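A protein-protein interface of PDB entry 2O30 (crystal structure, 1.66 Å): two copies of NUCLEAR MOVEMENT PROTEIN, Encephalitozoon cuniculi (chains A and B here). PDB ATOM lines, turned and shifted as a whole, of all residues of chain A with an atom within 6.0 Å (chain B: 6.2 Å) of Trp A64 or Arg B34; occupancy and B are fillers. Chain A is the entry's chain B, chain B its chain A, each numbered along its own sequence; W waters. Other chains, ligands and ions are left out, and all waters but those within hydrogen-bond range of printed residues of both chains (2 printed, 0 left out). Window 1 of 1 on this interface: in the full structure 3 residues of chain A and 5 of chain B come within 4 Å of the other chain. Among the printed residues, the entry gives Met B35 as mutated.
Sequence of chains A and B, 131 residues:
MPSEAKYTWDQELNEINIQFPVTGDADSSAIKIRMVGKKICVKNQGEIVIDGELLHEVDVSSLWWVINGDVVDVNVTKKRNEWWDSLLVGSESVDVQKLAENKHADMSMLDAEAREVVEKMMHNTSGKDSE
Among the printed residues, pairs that only touch across the chains: Trp A64 with Lys B32, Trp A64 with Ile B33, Trp A64 with Arg B34, Trp A64 with Cys B41 and Ile A67 with Val B36.
Printed residues of chain B within 4 Å of Trp A65: Arg B34. Printed residues of chain B within 4 Å of Ile A67: Val B36 (3.9 Å). Of the printed residues of chain A, Lys B32 touches Trp A64. Of the printed residues of chain A, Ile B33 touches Trp A64. Printed residues of chain A within 4 Å of Arg B34: Trp A64 and Trp A65. Met B35 touches none of the printed residues of chain A. Of the printed residues of chain A, Val B36 touches Ile A67. Leu B63 touches none of the printed residues of chain A. The nearest residue of chain B that does not touch Trp A64 is Lys B43 (4.1 Å). The nearest residue of chain A that does not touch Arg B34 is Val A66 (4.2 Å).
Of the 10 printed residues of chain A, 3 touch a printed residue of chain B. Printed residues of chain A that touch a printed residue of chain B: Trp A64, Trp A65 and Ile A67. Of the 11 printed residues of chain B, 5 touch a printed residue of chain A. Among the printed residues, 6 pairs touch across the chains. Among the printed residues, no Asp or Glu carboxylate lies within 4 Å of a Lys or Arg side-chain nitrogen of the other chain.
O of Lys B32 is in hydrogen-bond range of N of Lys B43 (2.8 Å). The backbone carbonyl oxygen of Arg B34 sits at hydrogen-bond distance from the backbone NH of Cys B41, 2.9 Å away. N of Asn A75 lies within hydrogen-bond range of O of Trp A64.
NH1 of Arg B34 is in hydrogen-bond range of O of Trp A65 (2.9 Å).
Water W2 bridges the side-chain amino group (NZ) of Lys B43 (2.8 Å) and the backbone carbonyl oxygen (O) of Leu A63 (2.8 Å). Water W1 bridges O of Leu A63 (2.9 Å) and NZ of Lys B43 (3.1 Å).
Position printed for both chains: 63.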
ATOM      1  N   SER A  62     -14.058  31.565 -28.464  1.00  0.00           N
ATOM      2  CA  SER A  62     -15.059  30.732 -27.786  1.00  0.00           C
ATOM      3  C   SER A  62     -14.550  29.296 -27.586  1.00  0.00           C
ATOM      4  O   SER A  62     -15.214  28.480 -26.938  1.00  0.00           O
ATOM      5  CB  SER A  62     -16.364  30.703 -28.580  1.00  0.00           C
ATOM      6  OG  SER A  62     -16.241  29.873 -29.729  1.00  0.00           O
ATOM      7  N   LEU A  63     -13.384  29.016 -28.150  1.00  0.00           N
ATOM      8  CA  LEU A  63     -12.776  27.672 -28.106  1.00  0.00           C
ATOM      9  C   LEU A  63     -12.655  27.217 -26.661  1.00  0.00           C
ATOM     10  O   LEU A  63     -12.162  27.951 -25.806  1.00  0.00           O
ATOM     11  CB  LEU A  63     -11.402  27.673 -28.786  1.00  0.00           C
ATOM     12  CG  LEU A  63     -10.607  26.363 -28.859  1.00  0.00           C
ATOM     13  CD1 LEU A  63     -11.387  25.313 -29.647  1.00  0.00           C
ATOM     14  CD2 LEU A  63      -9.200  26.589 -29.457  1.00  0.00           C
ATOM     15  N   TRP A  64     -13.119  26.008 -26.380  1.00  0.00           N
ATOM     16  CA  TRP A  64     -13.007  25.468 -25.024  1.00  0.00           C
ATOM     17  C   TRP A  64     -12.837  23.962 -25.124  1.00  0.00           C
ATOM     18  O   TRP A  64     -13.306  23.341 -26.059  1.00  0.00           O
ATOM     19  CB  TRP A  64     -14.261  25.800 -24.219  1.00  0.00           C
ATOM     20  CG  TRP A  64     -14.271  25.235 -22.825  1.00  0.00           C
ATOM     21  CD1 TRP A  64     -15.094  24.266 -22.346  1.00  0.00           C
ATOM     22  CD2 TRP A  64     -13.396  25.594 -21.746  1.00  0.00           C
ATOM     23  NE1 TRP A  64     -14.802  24.005 -21.020  1.00  0.00           N
ATOM     24  CE2 TRP A  64     -13.762  24.802 -20.631  1.00  0.00           C
ATOM     25  CE3 TRP A  64     -12.348  26.521 -21.608  1.00  0.00           C
ATOM     26  CZ2 TRP A  64     -13.102  24.890 -19.391  1.00  0.00           C
ATOM     27  CZ3 TRP A  64     -11.698  26.615 -20.363  1.00  0.00           C
ATOM     28  CH2 TRP A  64     -12.099  25.806 -19.274  1.00  0.00           C
ATOM     29  N   TRP A  65     -12.150  23.379 -24.155  1.00  0.00           N
ATOM     30  CA  TRP A  65     -12.049  21.927 -24.110  1.00  0.00           C
ATOM     31  C   TRP A  65     -11.934  21.442 -22.677  1.00  0.00           C
ATOM     32  O   TRP A  65     -11.534  22.188 -21.783  1.00  0.00           O
ATOM     33  CB  TRP A  65     -10.880  21.436 -24.942  1.00  0.00           C
ATOM     34  CG  TRP A  65      -9.518  21.907 -24.495  1.00  0.00           C
ATOM     35  CD1 TRP A  65      -8.904  23.073 -24.825  1.00  0.00           C
ATOM     36  CD2 TRP A  65      -8.604  21.193 -23.655  1.00  0.00           C
ATOM     37  NE1 TRP A  65      -7.648  23.139 -24.247  1.00  0.00           N
ATOM     38  CE2 TRP A  65      -7.448  21.992 -23.517  1.00  0.00           C
ATOM     39  CE3 TRP A  65      -8.646  19.942 -23.020  1.00  0.00           C
ATOM     40  CZ2 TRP A  65      -6.340  21.591 -22.752  1.00  0.00           C
ATOM     41  CZ3 TRP A  65      -7.541  19.536 -22.272  1.00  0.00           C
ATOM     42  CH2 TRP A  65      -6.409  20.368 -22.132  1.00  0.00           C
ATOM     43  N   VAL A  66     -12.338  20.196 -22.466  1.00  0.00           N
ATOM     44  CA  VAL A  66     -12.184  19.537 -21.182  1.00  0.00           C
ATOM     45  C   VAL A  66     -11.981  18.054 -21.414  1.00  0.00           C
ATOM     46  O   VAL A  66     -12.236  17.545 -22.516  1.00  0.00           O
ATOM     47  CB  VAL A  66     -13.423  19.693 -20.282  1.00  0.00           C
ATOM     48  CG1 VAL A  66     -13.529  21.124 -19.730  1.00  0.00           C
ATOM     49  CG2 VAL A  66     -14.687  19.245 -21.005  1.00  0.00           C
ATOM     50  N   ILE A  67     -11.526  17.362 -20.372  1.00  0.00           N
ATOM     51  CA  ILE A  67     -11.352  15.917 -20.437  1.00  0.00           C
ATOM     52  C   ILE A  67     -12.474  15.281 -19.628  1.00  0.00           C
ATOM     53  O   ILE A  67     -12.639  15.594 -18.439  1.00  0.00           O
ATOM     54  CB  ILE A  67      -9.967  15.484 -19.896  1.00  0.00           C
ATOM     55  CG1 ILE A  67      -8.844  16.101 -20.744  1.00  0.00           C
ATOM     56  CG2 ILE A  67      -9.879  13.955 -19.842  1.00  0.00           C
ATOM     57  CD1 ILE A  67      -7.432  15.908 -20.188  1.00  0.00           C
ATOM     58  N   ASP A  73     -13.192  16.588 -25.031  1.00  0.00           N
ATOM     59  CA  ASP A  73     -14.304  17.227 -25.749  1.00  0.00           C
ATOM     60  C   ASP A  73     -13.923  18.681 -26.048  1.00  0.00           C
ATOM     61  O   ASP A  73     -13.626  19.436 -25.140  1.00  0.00           O
ATOM     62  CB  ASP A  73     -15.574  17.156 -24.919  1.00  0.00           C
ATOM     63  CG  ASP A  73     -16.139  15.763 -24.843  1.00  0.00           C
ATOM     64  OD1 ASP A  73     -16.456  15.192 -25.904  1.00  0.00           O
ATOM     65  OD2 ASP A  73     -16.292  15.239 -23.729  1.00  0.00           O
ATOM     66  N   VAL A  74     -13.891  19.045 -27.327  1.00  0.00           N
ATOM     67  CA  VAL A  74     -13.536  20.408 -27.764  1.00  0.00           C
ATOM     68  C   VAL A  74     -14.793  21.040 -28.366  1.00  0.00           C
ATOM     69  O   VAL A  74     -15.535  20.381 -29.097  1.00  0.00           O
ATOM     70  CB  VAL A  74     -12.461  20.371 -28.852  1.00  0.00           C
ATOM     71  CG1 VAL A  74     -11.978  21.784 -29.215  1.00  0.00           C
ATOM     72  CG2 VAL A  74     -11.269  19.506 -28.408  1.00  0.00           C
ATOM     73  N   ASN A  75     -15.033  22.307 -28.052  1.00  0.00           N
ATOM     74  CA  ASN A  75     -16.242  22.992 -28.545  1.00  0.00           C
ATOM     75  C   ASN A  75     -15.813  24.373 -29.036  1.00  0.00           C
ATOM     76  O   ASN A  75     -14.978  25.019 -28.420  1.00  0.00           O
ATOM     77  CB  ASN A  75     -17.236  23.093 -27.386  1.00  0.00           C
ATOM     78  CG  ASN A  75     -18.380  24.002 -27.669  1.00  0.00           C
ATOM     79  OD1 ASN A  75     -18.337  25.196 -27.322  1.00  0.00           O
ATOM     80  ND2 ASN A  75     -19.417  23.469 -28.312  1.00  0.00           N
ATOM     81  N   VAL A  76     -16.379  24.823 -30.164  1.00  0.00           N
ATOM     82  CA  VAL A  76     -16.163  26.193 -30.623  1.00  0.00           C
ATOM     83  C   VAL A  76     -17.464  26.658 -31.297  1.00  0.00           C
ATOM     84  O   VAL A  76     -18.198  25.841 -31.879  1.00  0.00           O
ATOM     85  CB  VAL A  76     -14.924  26.332 -31.572  1.00  0.00           C
ATOM     86  CG1 VAL A  76     -15.090  25.550 -32.858  1.00  0.00           C
ATOM     87  CG2 VAL A  76     -14.607  27.819 -31.883  1.00  0.00           C
ATOM     88  N   LYS B  32     -16.608  28.364 -17.025  1.00  0.00           N
ATOM     89  CA  LYS B  32     -15.803  27.315 -17.627  1.00  0.00           C
ATOM     90  C   LYS B  32     -14.637  26.999 -16.701  1.00  0.00           C
ATOM     91  O   LYS B  32     -13.844  27.871 -16.407  1.00  0.00           O
ATOM     92  CB  LYS B  32     -15.302  27.768 -18.994  1.00  0.00           C
ATOM     93  CG  LYS B  32     -16.427  27.884 -20.044  1.00  0.00           C
ATOM     94  CD  LYS B  32     -15.845  28.300 -21.409  1.00  0.00           C
ATOM     95  CE  LYS B  32     -16.894  28.233 -22.540  1.00  0.00           C
ATOM     96  NZ  LYS B  32     -18.163  27.556 -22.128  1.00  0.00           N
ATOM     97  N   ILE B  33     -14.550  25.750 -16.250  1.00  0.00           N
ATOM     98  CA  ILE B  33     -13.497  25.329 -15.305  1.00  0.00           C
ATOM     99  C   ILE B  33     -12.854  24.042 -15.833  1.00  0.00           C
ATOM    100  O   ILE B  33     -13.555  23.075 -16.151  1.00  0.00           O
ATOM    101  CB  ILE B  33     -14.067  25.105 -13.882  1.00  0.00           C
ATOM    102  CG1 ILE B  33     -14.707  26.398 -13.375  1.00  0.00           C
ATOM    103  CG2 ILE B  33     -12.960  24.640 -12.918  1.00  0.00           C
ATOM    104  CD1 ILE B  33     -15.550  26.265 -12.095  1.00  0.00           C
ATOM    105  N   ARG B  34     -11.531  24.055 -15.954  1.00  0.00           N
ATOM    106  CA  ARG B  34     -10.763  22.871 -16.368  1.00  0.00           C
ATOM    107  C   ARG B  34      -9.518  22.740 -15.487  1.00  0.00           C
ATOM    108  O   ARG B  34      -8.798  23.713 -15.307  1.00  0.00           O
ATOM    109  CB  ARG B  34     -10.303  23.009 -17.817  1.00  0.00           C
ATOM    110  CG  ARG B  34      -9.449  21.839 -18.328  1.00  0.00           C
ATOM    111  CD  ARG B  34      -9.060  21.980 -19.807  1.00  0.00           C
ATOM    112  NE  ARG B  34      -8.116  23.067 -20.070  1.00  0.00           N
ATOM    113  CZ  ARG B  34      -8.367  24.136 -20.825  1.00  0.00           C
ATOM    114  NH1 ARG B  34      -9.537  24.288 -21.421  1.00  0.00           N
ATOM    115  NH2 ARG B  34      -7.433  25.061 -20.999  1.00  0.00           N
ATOM    116  N   MET B  35      -9.264  21.536 -14.977  1.00  0.00           N
ATOM    117  CA  MET B  35      -7.991  21.229 -14.367  1.00  0.00           C
ATOM    118  C   MET B  35      -7.432  20.003 -15.081  1.00  0.00           C
ATOM    119  O   MET B  35      -8.157  19.024 -15.275  1.00  0.00           O
ATOM    120  CB  MET B  35      -8.156  20.943 -12.870  1.00  0.00           C
ATOM    121  CG  MET B  35      -8.527  22.139 -12.009  1.00  0.00           C
ATOM    122  SD  MET B  35      -8.258  21.749 -10.240  1.00  0.00           S
ATOM    123  CE  MET B  35      -6.522  21.454 -10.394  1.00  0.00           C
ATOM    124  N   VAL B  36      -6.163  20.076 -15.472  1.00  0.00           N
ATOM    125  CA  VAL B  36      -5.418  18.939 -16.008  1.00  0.00           C
ATOM    126  C   VAL B  36      -4.075  18.923 -15.285  1.00  0.00           C
ATOM    127  O   VAL B  36      -3.290  19.880 -15.391  1.00  0.00           O
ATOM    128  CB  VAL B  36      -5.172  19.047 -17.537  1.00  0.00           C
ATOM    129  CG1 VAL B  36      -4.435  17.802 -18.055  1.00  0.00           C
ATOM    130  CG2 VAL B  36      -6.490  19.214 -18.271  1.00  0.00           C
ATOM    131  N   LYS B  39      -2.488  22.153 -13.692  1.00  0.00           N
ATOM    132  CA  LYS B  39      -2.894  23.298 -14.508  1.00  0.00           C
ATOM    133  C   LYS B  39      -4.366  23.583 -14.274  1.00  0.00           C
ATOM    134  O   LYS B  39      -5.198  22.683 -14.317  1.00  0.00           O
ATOM    135  CB  LYS B  39      -2.644  23.023 -15.999  1.00  0.00           C
ATOM    136  CG  LYS B  39      -1.186  22.721 -16.373  1.00  0.00           C
ATOM    137  CD  LYS B  39      -0.310  23.972 -16.328  1.00  0.00           C
ATOM    138  CE  LYS B  39       1.168  23.640 -16.606  1.00  0.00           C
ATOM    139  NZ  LYS B  39       2.069  24.718 -16.076  1.00  0.00           N
ATOM    140  N   ILE B  40      -4.684  24.840 -14.014  1.00  0.00           N
ATOM    141  CA  ILE B  40      -6.053  25.227 -13.738  1.00  0.00           C
ATOM    142  C   ILE B  40      -6.428  26.431 -14.612  1.00  0.00           C
ATOM    143  O   ILE B  40      -5.669  27.379 -14.753  1.00  0.00           O
ATOM    144  CB  ILE B  40      -6.238  25.541 -12.236  1.00  0.00           C
ATOM    145  CG1 ILE B  40      -7.667  26.049 -11.953  1.00  0.00           C
ATOM    146  CG2 ILE B  40      -5.149  26.509 -11.764  1.00  0.00           C
ATOM    147  CD1 ILE B  40      -7.930  26.347 -10.466  1.00  0.00           C
ATOM    148  N   CYS B  41      -7.595  26.336 -15.235  1.00  0.00           N
ATOM    149  CA  CYS B  41      -8.156  27.410 -16.043  1.00  0.00           C
ATOM    150  C   CYS B  41      -9.593  27.628 -15.590  1.00  0.00           C
ATOM    151  O   CYS B  41     -10.402  26.697 -15.611  1.00  0.00           O
ATOM    152  CB  CYS B  41      -8.159  27.007 -17.515  1.00  0.00           C
ATOM    153  SG  CYS B  41      -8.937  28.277 -18.547  1.00  0.00           S
ATOM    154  N   VAL B  42      -9.904  28.848 -15.159  1.00  0.00           N
ATOM    155  CA  VAL B  42     -11.268  29.207 -14.778  1.00  0.00           C
ATOM    156  C   VAL B  42     -11.629  30.464 -15.559  1.00  0.00           C
ATOM    157  O   VAL B  42     -10.925  31.460 -15.496  1.00  0.00           O
ATOM    158  CB  VAL B  42     -11.390  29.484 -13.252  1.00  0.00           C
ATOM    159  CG1 VAL B  42     -12.805  29.978 -12.897  1.00  0.00           C
ATOM    160  CG2 VAL B  42     -11.030  28.223 -12.448  1.00  0.00           C
ATOM    161  N   LYS B  43     -12.721  30.403 -16.300  1.00  0.00           N
ATOM    162  CA  LYS B  43     -13.177  31.575 -17.041  1.00  0.00           C
ATOM    163  C   LYS B  43     -14.618  31.885 -16.697  1.00  0.00           C
ATOM    164  O   LYS B  43     -15.387  30.996 -16.380  1.00  0.00           O
ATOM    165  CB  LYS B  43     -13.011  31.358 -18.542  1.00  0.00           C
ATOM    166  CG  LYS B  43     -11.582  31.050 -18.943  1.00  0.00           C
ATOM    167  CD  LYS B  43     -11.284  31.509 -20.358  1.00  0.00           C
ATOM    168  CE  LYS B  43     -11.949  30.638 -21.385  1.00  0.00           C
ATOM    169  NZ  LYS B  43     -11.304  30.859 -22.721  1.00  0.00           N
ATOM    170  N   LEU B  63     -12.915  17.503  -8.273  1.00  0.00           N
ATOM    171  CA  LEU B  63     -13.280  18.904  -8.586  1.00  0.00           C
ATOM    172  C   LEU B  63     -14.792  19.082  -8.644  1.00  0.00           C
ATOM    173  O   LEU B  63     -15.484  18.319  -9.314  1.00  0.00           O
ATOM    174  CB  LEU B  63     -12.661  19.328  -9.917  1.00  0.00           C
ATOM    175  CG  LEU B  63     -12.917  20.749 -10.426  1.00  0.00           C
ATOM    176  CD1 LEU B  63     -12.453  21.746  -9.409  1.00  0.00           C
ATOM    177  CD2 LEU B  63     -12.196  20.956 -11.762  1.00  0.00           C
HETATM  178  O   HOH W   1     -10.544  30.336 -25.666  1.00  0.00           O
HETATM  179  O   HOH W   2     -13.517  29.653 -23.990  1.00  0.00           O
